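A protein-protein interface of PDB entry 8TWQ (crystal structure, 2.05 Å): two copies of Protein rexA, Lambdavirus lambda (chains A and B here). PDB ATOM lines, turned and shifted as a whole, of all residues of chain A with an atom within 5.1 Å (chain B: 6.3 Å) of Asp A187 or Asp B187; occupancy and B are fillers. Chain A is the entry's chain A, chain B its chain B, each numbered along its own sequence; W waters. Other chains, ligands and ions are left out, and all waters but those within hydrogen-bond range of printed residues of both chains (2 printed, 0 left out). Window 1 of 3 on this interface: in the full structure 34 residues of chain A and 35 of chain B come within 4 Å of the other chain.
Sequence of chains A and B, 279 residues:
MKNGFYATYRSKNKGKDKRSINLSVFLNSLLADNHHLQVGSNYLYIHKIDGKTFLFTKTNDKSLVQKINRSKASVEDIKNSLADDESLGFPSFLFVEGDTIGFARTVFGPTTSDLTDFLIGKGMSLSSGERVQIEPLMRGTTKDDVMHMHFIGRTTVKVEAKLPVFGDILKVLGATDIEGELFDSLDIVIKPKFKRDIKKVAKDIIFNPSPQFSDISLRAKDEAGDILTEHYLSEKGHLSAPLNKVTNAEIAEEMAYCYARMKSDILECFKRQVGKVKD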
ATOM      1  N   THR A 156      -0.327 -10.536  21.819  1.00  0.00           N
ATOM      2  CA  THR A 156      -0.323 -10.950  20.414  1.00  0.00           C
ATOM      3  C   THR A 156       0.189 -12.373  20.267  1.00  0.00           C
ATOM      4  O   THR A 156       1.337 -12.663  20.608  1.00  0.00           O
ATOM      5  CB  THR A 156       0.533 -10.029  19.556  1.00  0.00           C
ATOM      6  OG1 THR A 156       0.085  -8.684  19.716  1.00  0.00           O
ATOM      7  CG2 THR A 156       0.421 -10.448  18.084  1.00  0.00           C
ATOM      8  N   VAL A 157      -0.651 -13.238  19.721  1.00  0.00           N
ATOM      9  CA  VAL A 157      -0.358 -14.653  19.535  1.00  0.00           C
ATOM     10  C   VAL A 157       0.046 -14.832  18.084  1.00  0.00           C
ATOM     11  O   VAL A 157      -0.783 -14.672  17.182  1.00  0.00           O
ATOM     12  CB  VAL A 157      -1.575 -15.531  19.858  1.00  0.00           C
ATOM     13  CG1 VAL A 157      -1.238 -16.997  19.641  1.00  0.00           C
ATOM     14  CG2 VAL A 157      -2.080 -15.274  21.273  1.00  0.00           C
ATOM     15  N   LYS A 158       1.306 -15.162  17.833  1.00  0.00           N
ATOM     16  CA  LYS A 158       1.728 -15.410  16.467  1.00  0.00           C
ATOM     17  C   LYS A 158       1.549 -16.891  16.163  1.00  0.00           C
ATOM     18  O   LYS A 158       1.914 -17.747  16.975  1.00  0.00           O
ATOM     19  CB  LYS A 158       3.173 -14.988  16.230  1.00  0.00           C
ATOM     20  CG  LYS A 158       3.602 -15.290  14.786  1.00  0.00           C
ATOM     21  CD  LYS A 158       5.111 -15.320  14.608  1.00  0.00           C
ATOM     22  CE  LYS A 158       5.515 -14.384  13.476  1.00  0.00           C
ATOM     23  NZ  LYS A 158       4.846 -13.043  13.589  1.00  0.00           N
ATOM     24  N   VAL A 159       0.958 -17.190  15.016  1.00  0.00           N
ATOM     25  CA  VAL A 159       0.723 -18.569  14.600  1.00  0.00           C
ATOM     26  C   VAL A 159       1.337 -18.745  13.213  1.00  0.00           C
ATOM     27  O   VAL A 159       0.742 -18.333  12.212  1.00  0.00           O
ATOM     28  CB  VAL A 159      -0.770 -18.926  14.590  1.00  0.00           C
ATOM     29  CG1 VAL A 159      -0.964 -20.401  14.227  1.00  0.00           C
ATOM     30  CG2 VAL A 159      -1.409 -18.593  15.925  1.00  0.00           C
ATOM     31  N   SER A 185       1.880 -16.315   8.340  1.00  0.00           N
ATOM     32  CA  SER A 185       1.358 -16.558   9.675  1.00  0.00           C
ATOM     33  C   SER A 185       0.090 -15.732   9.830  1.00  0.00           C
ATOM     34  O   SER A 185      -0.365 -15.064   8.897  1.00  0.00           O
ATOM     35  CB  SER A 185       2.390 -16.208  10.750  1.00  0.00           C
ATOM     36  OG  SER A 185       2.675 -14.824  10.755  1.00  0.00           O
ATOM     37  N   LEU A 186      -0.504 -15.828  11.005  1.00  0.00           N
ATOM     38  CA  LEU A 186      -1.484 -14.863  11.462  1.00  0.00           C
ATOM     39  C   LEU A 186      -1.099 -14.450  12.878  1.00  0.00           C
ATOM     40  O   LEU A 186      -0.369 -15.162  13.580  1.00  0.00           O
ATOM     41  CB  LEU A 186      -2.916 -15.420  11.395  1.00  0.00           C
ATOM     42  CG  LEU A 186      -3.271 -16.725  12.129  1.00  0.00           C
ATOM     43  CD1 LEU A 186      -3.484 -16.498  13.623  1.00  0.00           C
ATOM     44  CD2 LEU A 186      -4.496 -17.369  11.512  1.00  0.00           C
ATOM     45  N   ASP A 187      -1.563 -13.265  13.278  1.00  0.00           N
ATOM     46  CA  ASP A 187      -1.461 -12.795  14.654  1.00  0.00           C
ATOM     47  C   ASP A 187      -2.859 -12.642  15.226  1.00  0.00           C
ATOM     48  O   ASP A 187      -3.759 -12.129  14.553  1.00  0.00           O
ATOM     49  CB  ASP A 187      -0.747 -11.436  14.771  1.00  0.00           C
ATOM     50  CG  ASP A 187       0.727 -11.493  14.412  1.00  0.00           C
ATOM     51  OD1 ASP A 187       1.360 -12.563  14.547  1.00  0.00           O
ATOM     52  OD2 ASP A 187       1.256 -10.436  14.004  1.00  0.00           O
ATOM     53  N   ILE A 188      -3.037 -13.069  16.471  1.00  0.00           N
ATOM     54  CA  ILE A 188      -4.251 -12.788  17.231  1.00  0.00           C
ATOM     55  C   ILE A 188      -3.893 -11.686  18.217  1.00  0.00           C
ATOM     56  O   ILE A 188      -3.265 -11.940  19.249  1.00  0.00           O
ATOM     57  CB  ILE A 188      -4.781 -14.031  17.943  1.00  0.00           C
ATOM     58  CG1 ILE A 188      -4.959 -15.178  16.948  1.00  0.00           C
ATOM     59  CG2 ILE A 188      -6.085 -13.723  18.613  1.00  0.00           C
ATOM     60  CD1 ILE A 188      -4.281 -16.435  17.410  1.00  0.00           C
ATOM     61  N   VAL A 189      -4.272 -10.452  17.887  1.00  0.00           N
ATOM     62  CA  VAL A 189      -4.002  -9.295  18.739  1.00  0.00           C
ATOM     63  C   VAL A 189      -5.161  -9.171  19.721  1.00  0.00           C
ATOM     64  O   VAL A 189      -6.277  -8.852  19.323  1.00  0.00           O
ATOM     65  CB  VAL A 189      -3.832  -8.010  17.913  1.00  0.00           C
ATOM     66  CG1 VAL A 189      -3.430  -6.842  18.801  1.00  0.00           C
ATOM     67  CG2 VAL A 189      -2.791  -8.208  16.826  1.00  0.00           C
ATOM     68  N   LYS A 191      -6.927  -7.305  22.567  1.00  0.00           N
ATOM     69  CA  LYS A 191      -6.989  -5.961  23.119  1.00  0.00           C
ATOM     70  C   LYS A 191      -7.968  -5.871  24.288  1.00  0.00           C
ATOM     71  O   LYS A 191      -9.183  -6.014  24.088  1.00  0.00           O
ATOM     72  CB  LYS A 191      -7.380  -4.997  22.002  1.00  0.00           C
ATOM     73  CG  LYS A 191      -6.505  -5.196  20.754  1.00  0.00           C
ATOM     74  CD  LYS A 191      -7.118  -4.591  19.460  1.00  0.00           C
ATOM     75  CE  LYS A 191      -6.062  -3.852  18.585  1.00  0.00           C
ATOM     76  NZ  LYS A 191      -6.655  -2.917  17.548  1.00  0.00           N
ATOM     77  N   SER A 264       7.600  -8.720  11.476  1.00  0.00           N
ATOM     78  CA  SER A 264       6.380  -7.934  11.610  1.00  0.00           C
ATOM     79  C   SER A 264       6.295  -7.219  12.954  1.00  0.00           C
ATOM     80  O   SER A 264       6.144  -5.995  13.015  1.00  0.00           O
ATOM     81  CB  SER A 264       5.186  -8.867  11.441  1.00  0.00           C
ATOM     82  OG  SER A 264       5.486  -9.866  10.477  1.00  0.00           O
ATOM     83  N   ASP A 265       6.406  -7.975  14.045  1.00  0.00           N
ATOM     84  CA  ASP A 265       6.170  -7.419  15.375  1.00  0.00           C
ATOM     85  C   ASP A 265       7.220  -6.381  15.753  1.00  0.00           C
ATOM     86  O   ASP A 265       6.903  -5.385  16.420  1.00  0.00           O
ATOM     87  CB  ASP A 265       6.147  -8.546  16.406  1.00  0.00           C
ATOM     88  CG  ASP A 265       4.977  -9.483  16.213  1.00  0.00           C
ATOM     89  OD1 ASP A 265       5.007 -10.318  15.265  1.00  0.00           O
ATOM     90  OD2 ASP A 265       4.029  -9.366  17.021  1.00  0.00           O
ATOM     91  N   THR B 156      -6.939  -8.009   7.771  1.00  0.00           N
ATOM     92  CA  THR B 156      -7.037  -7.855   9.215  1.00  0.00           C
ATOM     93  C   THR B 156      -8.506  -7.945   9.597  1.00  0.00           C
ATOM     94  O   THR B 156      -9.311  -7.108   9.176  1.00  0.00           O
ATOM     95  CB  THR B 156      -6.448  -6.519   9.673  1.00  0.00           C
ATOM     96  OG1 THR B 156      -5.044  -6.508   9.406  1.00  0.00           O
ATOM     97  CG2 THR B 156      -6.681  -6.303  11.181  1.00  0.00           C
ATOM     98  N   VAL B 157      -8.852  -8.953  10.381  1.00  0.00           N
ATOM     99  CA  VAL B 157     -10.233  -9.236  10.735  1.00  0.00           C
ATOM    100  C   VAL B 157     -10.416  -8.810  12.180  1.00  0.00           C
ATOM    101  O   VAL B 157      -9.782  -9.362  13.082  1.00  0.00           O
ATOM    102  CB  VAL B 157     -10.555 -10.718  10.518  1.00  0.00           C
ATOM    103  CG1 VAL B 157     -12.008 -11.054  10.903  1.00  0.00           C
ATOM    104  CG2 VAL B 157     -10.264 -11.084   9.058  1.00  0.00           C
ATOM    105  N   LYS B 158     -11.254  -7.800  12.394  1.00  0.00           N
ATOM    106  CA  LYS B 158     -11.510  -7.248  13.716  1.00  0.00           C
ATOM    107  C   LYS B 158     -12.801  -7.834  14.267  1.00  0.00           C
ATOM    108  O   LYS B 158     -13.819  -7.856  13.574  1.00  0.00           O
ATOM    109  CB  LYS B 158     -11.609  -5.725  13.651  1.00  0.00           C
ATOM    110  CG  LYS B 158     -10.700  -5.132  12.586  1.00  0.00           C
ATOM    111  CD  LYS B 158     -10.677  -3.605  12.617  1.00  0.00           C
ATOM    112  CE  LYS B 158      -9.672  -3.046  11.594  1.00  0.00           C
ATOM    113  NZ  LYS B 158      -8.252  -3.279  12.002  1.00  0.00           N
ATOM    114  N   VAL B 159     -12.755  -8.305  15.511  1.00  0.00           N
ATOM    115  CA  VAL B 159     -13.892  -8.962  16.156  1.00  0.00           C
ATOM    116  C   VAL B 159     -14.173  -8.263  17.490  1.00  0.00           C
ATOM    117  O   VAL B 159     -13.385  -8.384  18.431  1.00  0.00           O
ATOM    118  CB  VAL B 159     -13.635 -10.461  16.369  1.00  0.00           C
ATOM    119  CG1 VAL B 159     -14.815 -11.091  17.105  1.00  0.00           C
ATOM    120  CG2 VAL B 159     -13.391 -11.166  15.031  1.00  0.00           C
ATOM    121  N   SER B 185     -11.683  -6.121  22.035  1.00  0.00           N
ATOM    122  CA  SER B 185     -11.765  -6.785  20.737  1.00  0.00           C
ATOM    123  C   SER B 185     -10.538  -7.665  20.554  1.00  0.00           C
ATOM    124  O   SER B 185      -9.628  -7.675  21.381  1.00  0.00           O
ATOM    125  CB  SER B 185     -11.858  -5.772  19.592  1.00  0.00           C
ATOM    126  OG  SER B 185     -10.768  -4.863  19.668  1.00  0.00           O
ATOM    127  N   LEU B 186     -10.541  -8.415  19.460  1.00  0.00           N
ATOM    128  CA  LEU B 186      -9.333  -9.063  18.967  1.00  0.00           C
ATOM    129  C   LEU B 186      -9.265  -8.873  17.461  1.00  0.00           C
ATOM    130  O   LEU B 186     -10.299  -8.764  16.791  1.00  0.00           O
ATOM    131  CB  LEU B 186      -9.250 -10.569  19.334  1.00  0.00           C
ATOM    132  CG  LEU B 186     -10.221 -11.649  18.795  1.00  0.00           C
ATOM    133  CD1 LEU B 186      -9.948 -12.078  17.365  1.00  0.00           C
ATOM    134  CD2 LEU B 186     -10.191 -12.865  19.705  1.00  0.00           C
ATOM    135  N   ASP B 187      -8.034  -8.816  16.940  1.00  0.00           N
ATOM    136  CA  ASP B 187      -7.777  -8.798  15.508  1.00  0.00           C
ATOM    137  C   ASP B 187      -7.052 -10.069  15.078  1.00  0.00           C
ATOM    138  O   ASP B 187      -6.144 -10.541  15.768  1.00  0.00           O
ATOM    139  CB  ASP B 187      -6.931  -7.588  15.106  1.00  0.00           C
ATOM    140  CG  ASP B 187      -7.608  -6.277  15.403  1.00  0.00           C
ATOM    141  OD1 ASP B 187      -8.817  -6.135  15.131  1.00  0.00           O
ATOM    142  OD2 ASP B 187      -6.929  -5.376  15.925  1.00  0.00           O
ATOM    143  N   ILE B 188      -7.468 -10.618  13.937  1.00  0.00           N
ATOM    144  CA  ILE B 188      -6.736 -11.653  13.217  1.00  0.00           C
ATOM    145  C   ILE B 188      -6.067 -10.989  12.025  1.00  0.00           C
ATOM    146  O   ILE B 188      -6.720 -10.656  11.026  1.00  0.00           O
ATOM    147  CB  ILE B 188      -7.645 -12.799  12.753  1.00  0.00           C
ATOM    148  CG1 ILE B 188      -8.518 -13.309  13.906  1.00  0.00           C
ATOM    149  CG2 ILE B 188      -6.805 -13.940  12.145  1.00  0.00           C
ATOM    150  CD1 ILE B 188      -9.993 -13.159  13.634  1.00  0.00           C
ATOM    151  N   VAL B 189      -4.755 -10.812  12.130  1.00  0.00           N
ATOM    152  CA  VAL B 189      -3.956 -10.248  11.049  1.00  0.00           C
ATOM    153  C   VAL B 189      -3.421 -11.406  10.211  1.00  0.00           C
ATOM    154  O   VAL B 189      -2.567 -12.173  10.657  1.00  0.00           O
ATOM    155  CB  VAL B 189      -2.823  -9.362  11.589  1.00  0.00           C
ATOM    156  CG1 VAL B 189      -2.195  -8.549  10.439  1.00  0.00           C
ATOM    157  CG2 VAL B 189      -3.344  -8.442  12.704  1.00  0.00           C
ATOM    158  N   ILE B 190      -3.921 -11.532   8.997  1.00  0.00           N
ATOM    159  CA  ILE B 190      -3.582 -12.641   8.124  1.00  0.00           C
ATOM    160  C   ILE B 190      -2.526 -12.157   7.157  1.00  0.00           C
ATOM    161  O   ILE B 190      -2.831 -11.386   6.242  1.00  0.00           O
ATOM    162  CB  ILE B 190      -4.808 -13.149   7.376  1.00  0.00           C
ATOM    163  CG1 ILE B 190      -5.928 -13.434   8.388  1.00  0.00           C
ATOM    164  CG2 ILE B 190      -4.415 -14.354   6.537  1.00  0.00           C
ATOM    165  CD1 ILE B 190      -7.246 -13.655   7.739  1.00  0.00           C
ATOM    166  N   LYS B 191      -1.292 -12.617   7.345  1.00  0.00           N
ATOM    167  CA  LYS B 191      -0.143 -12.068   6.634  1.00  0.00           C
ATOM    168  C   LYS B 191       0.281 -13.004   5.515  1.00  0.00           C
ATOM    169  O   LYS B 191       0.684 -14.143   5.803  1.00  0.00           O
ATOM    170  CB  LYS B 191       1.011 -11.850   7.604  1.00  0.00           C
ATOM    171  CG  LYS B 191       0.642 -10.970   8.776  1.00  0.00           C
ATOM    172  CD  LYS B 191       1.844 -10.695   9.658  1.00  0.00           C
ATOM    173  CE  LYS B 191       2.174 -11.885  10.541  1.00  0.00           C
ATOM    174  NZ  LYS B 191       3.362 -11.660  11.450  1.00  0.00           N
HETATM  175  O   HOH W   1      -9.673  -4.346  16.874  1.00  0.00           O
HETATM  176  O   HOH W   2      -7.866  -1.459  14.613  1.00  0.00           O
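The backbone carbonyl oxygen (O) of Ser A185 sits at hydrogen-bond distance from the backbone NH (N) of Lys B191, at 3.0 Å. The backbone carbonyl oxygen of Asp A187 sits at hydrogen-bond distance from the backbone NH of Val B189, at 2.9 Å. OD2 of Asp A187 is in salt-bridge range of NZ of Lys B191 (3.5 Å). The backbone NH of Val A189 sits at hydrogen-bond distance from the backbone carbonyl oxygen of Asp B187, at 2.8 Å. The backbone NH (N) of Lys A191 sits at hydrogen-bond distance from the backbone carbonyl oxygen (O) of Ser B185 (3.0 Å). The side-chain amino group (NZ) of Lys A191 is in salt-bridge range of the side-chain carboxylate (OD2) of Asp B187. The side-chain amino group (NZ) of Lys B191 is in hydrogen-bond range of the side-chain hydroxyl (OG) of Ser A264, 2.9 Å away. The side-chain amino group of Lys A158 sits close to the side-chain amino group of Lys B191 (2.9 Å). O of Asp A187 sits close to O of Asp B187 (3.1 Å).
The backbone NH of Ile A188 is in hydrogen-bond range of the backbone carbonyl oxygen of Val A157, at 2.9 Å. The side-chain amino group (NZ) of Lys A158 lies within salt-bridge range of the side-chain carboxylate (OD1) of Asp A187, 3.6 Å away. NZ of Lys A158 is in salt-bridge range of OD1 of Asp A265, at 3.2 Å. N of Val A159 sits at hydrogen-bond distance from O of Leu A186, 2.8 Å away. The backbone carbonyl oxygen (O) of Val B157 lies within hydrogen-bond range of the backbone NH (N) of Ile B188 (2.8 Å). The backbone NH of Val B159 lies within hydrogen-bond range of the backbone carbonyl oxygen of Leu B186, 2.8 Å away.
Leu A186 touches Val B189. Asp A187 touches Ile B188. O of Asp B187 touches CA of Ile A188 (3.3 Å). Leu B186 touches Val A189 (CA to O, 3.1 Å).
Of the printed residues of chain B, Asp A187 touches Asp B187 (3.1 Å), Ile B188 (3.3 Å), Val B189 (2.9 Å) and Lys B191 (3.5 Å). Asp B187 touches four residues of chain A. Of the printed residues of chain B, Ser A185 touches Lys B191. Of the printed residues of chain B, Ile A188 touches Asp B187. The nearest residue of chain B that does not touch Asp A187 is Ile B190 (5.2 Å). The nearest printed residue of chain A that does not touch Asp B187 is Leu A186 (6.9 Å).
Printed residues of chain B that touch a printed residue of chain A: Ser B185, Leu B186, Asp B187, Ile B188, Val B189 and Lys B191. Hydrophobic or aromatic side chains of chain B that line the printed part of chain A: Leu B186. Among the printed residues, 13 pairs touch across the chains. Among the printed residues, Asp or Glu carboxylates within 4 Å of a Lys or Arg side-chain nitrogen of the other chain: Asp A187 with Lys B191 (3.5 Å) and Lys A191 with Asp B187 (3.0 Å).
Ser A185 touches Lys B191, and with the chains exchanged Lys A191 touches Ser B185. Asp A187 touches its own counterpart, Asp B187. Asp A187 touches Val B189, and with the chains exchanged Val A189 touches Asp B187. Asp A187 touches Lys B191, and with the chains exchanged Lys A191 touches Asp B187. Of the 13 pairs that touch across the chains among the printed residues, 11 have their exchanged pair printed and touching as well.
Water W1 lies within hydrogen-bond range of the side-chain carboxylate (OD1) of Asp B187 (2.6 Å), the side-chain hydroxyl (OG) of Ser B185 (3.0 Å) and the side-chain amino group (NZ) of Lys A191 (3.4 Å). Water W2 bridges NZ of Lys B158 (3.2 Å) and NZ of Lys A191 (3.5 Å).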
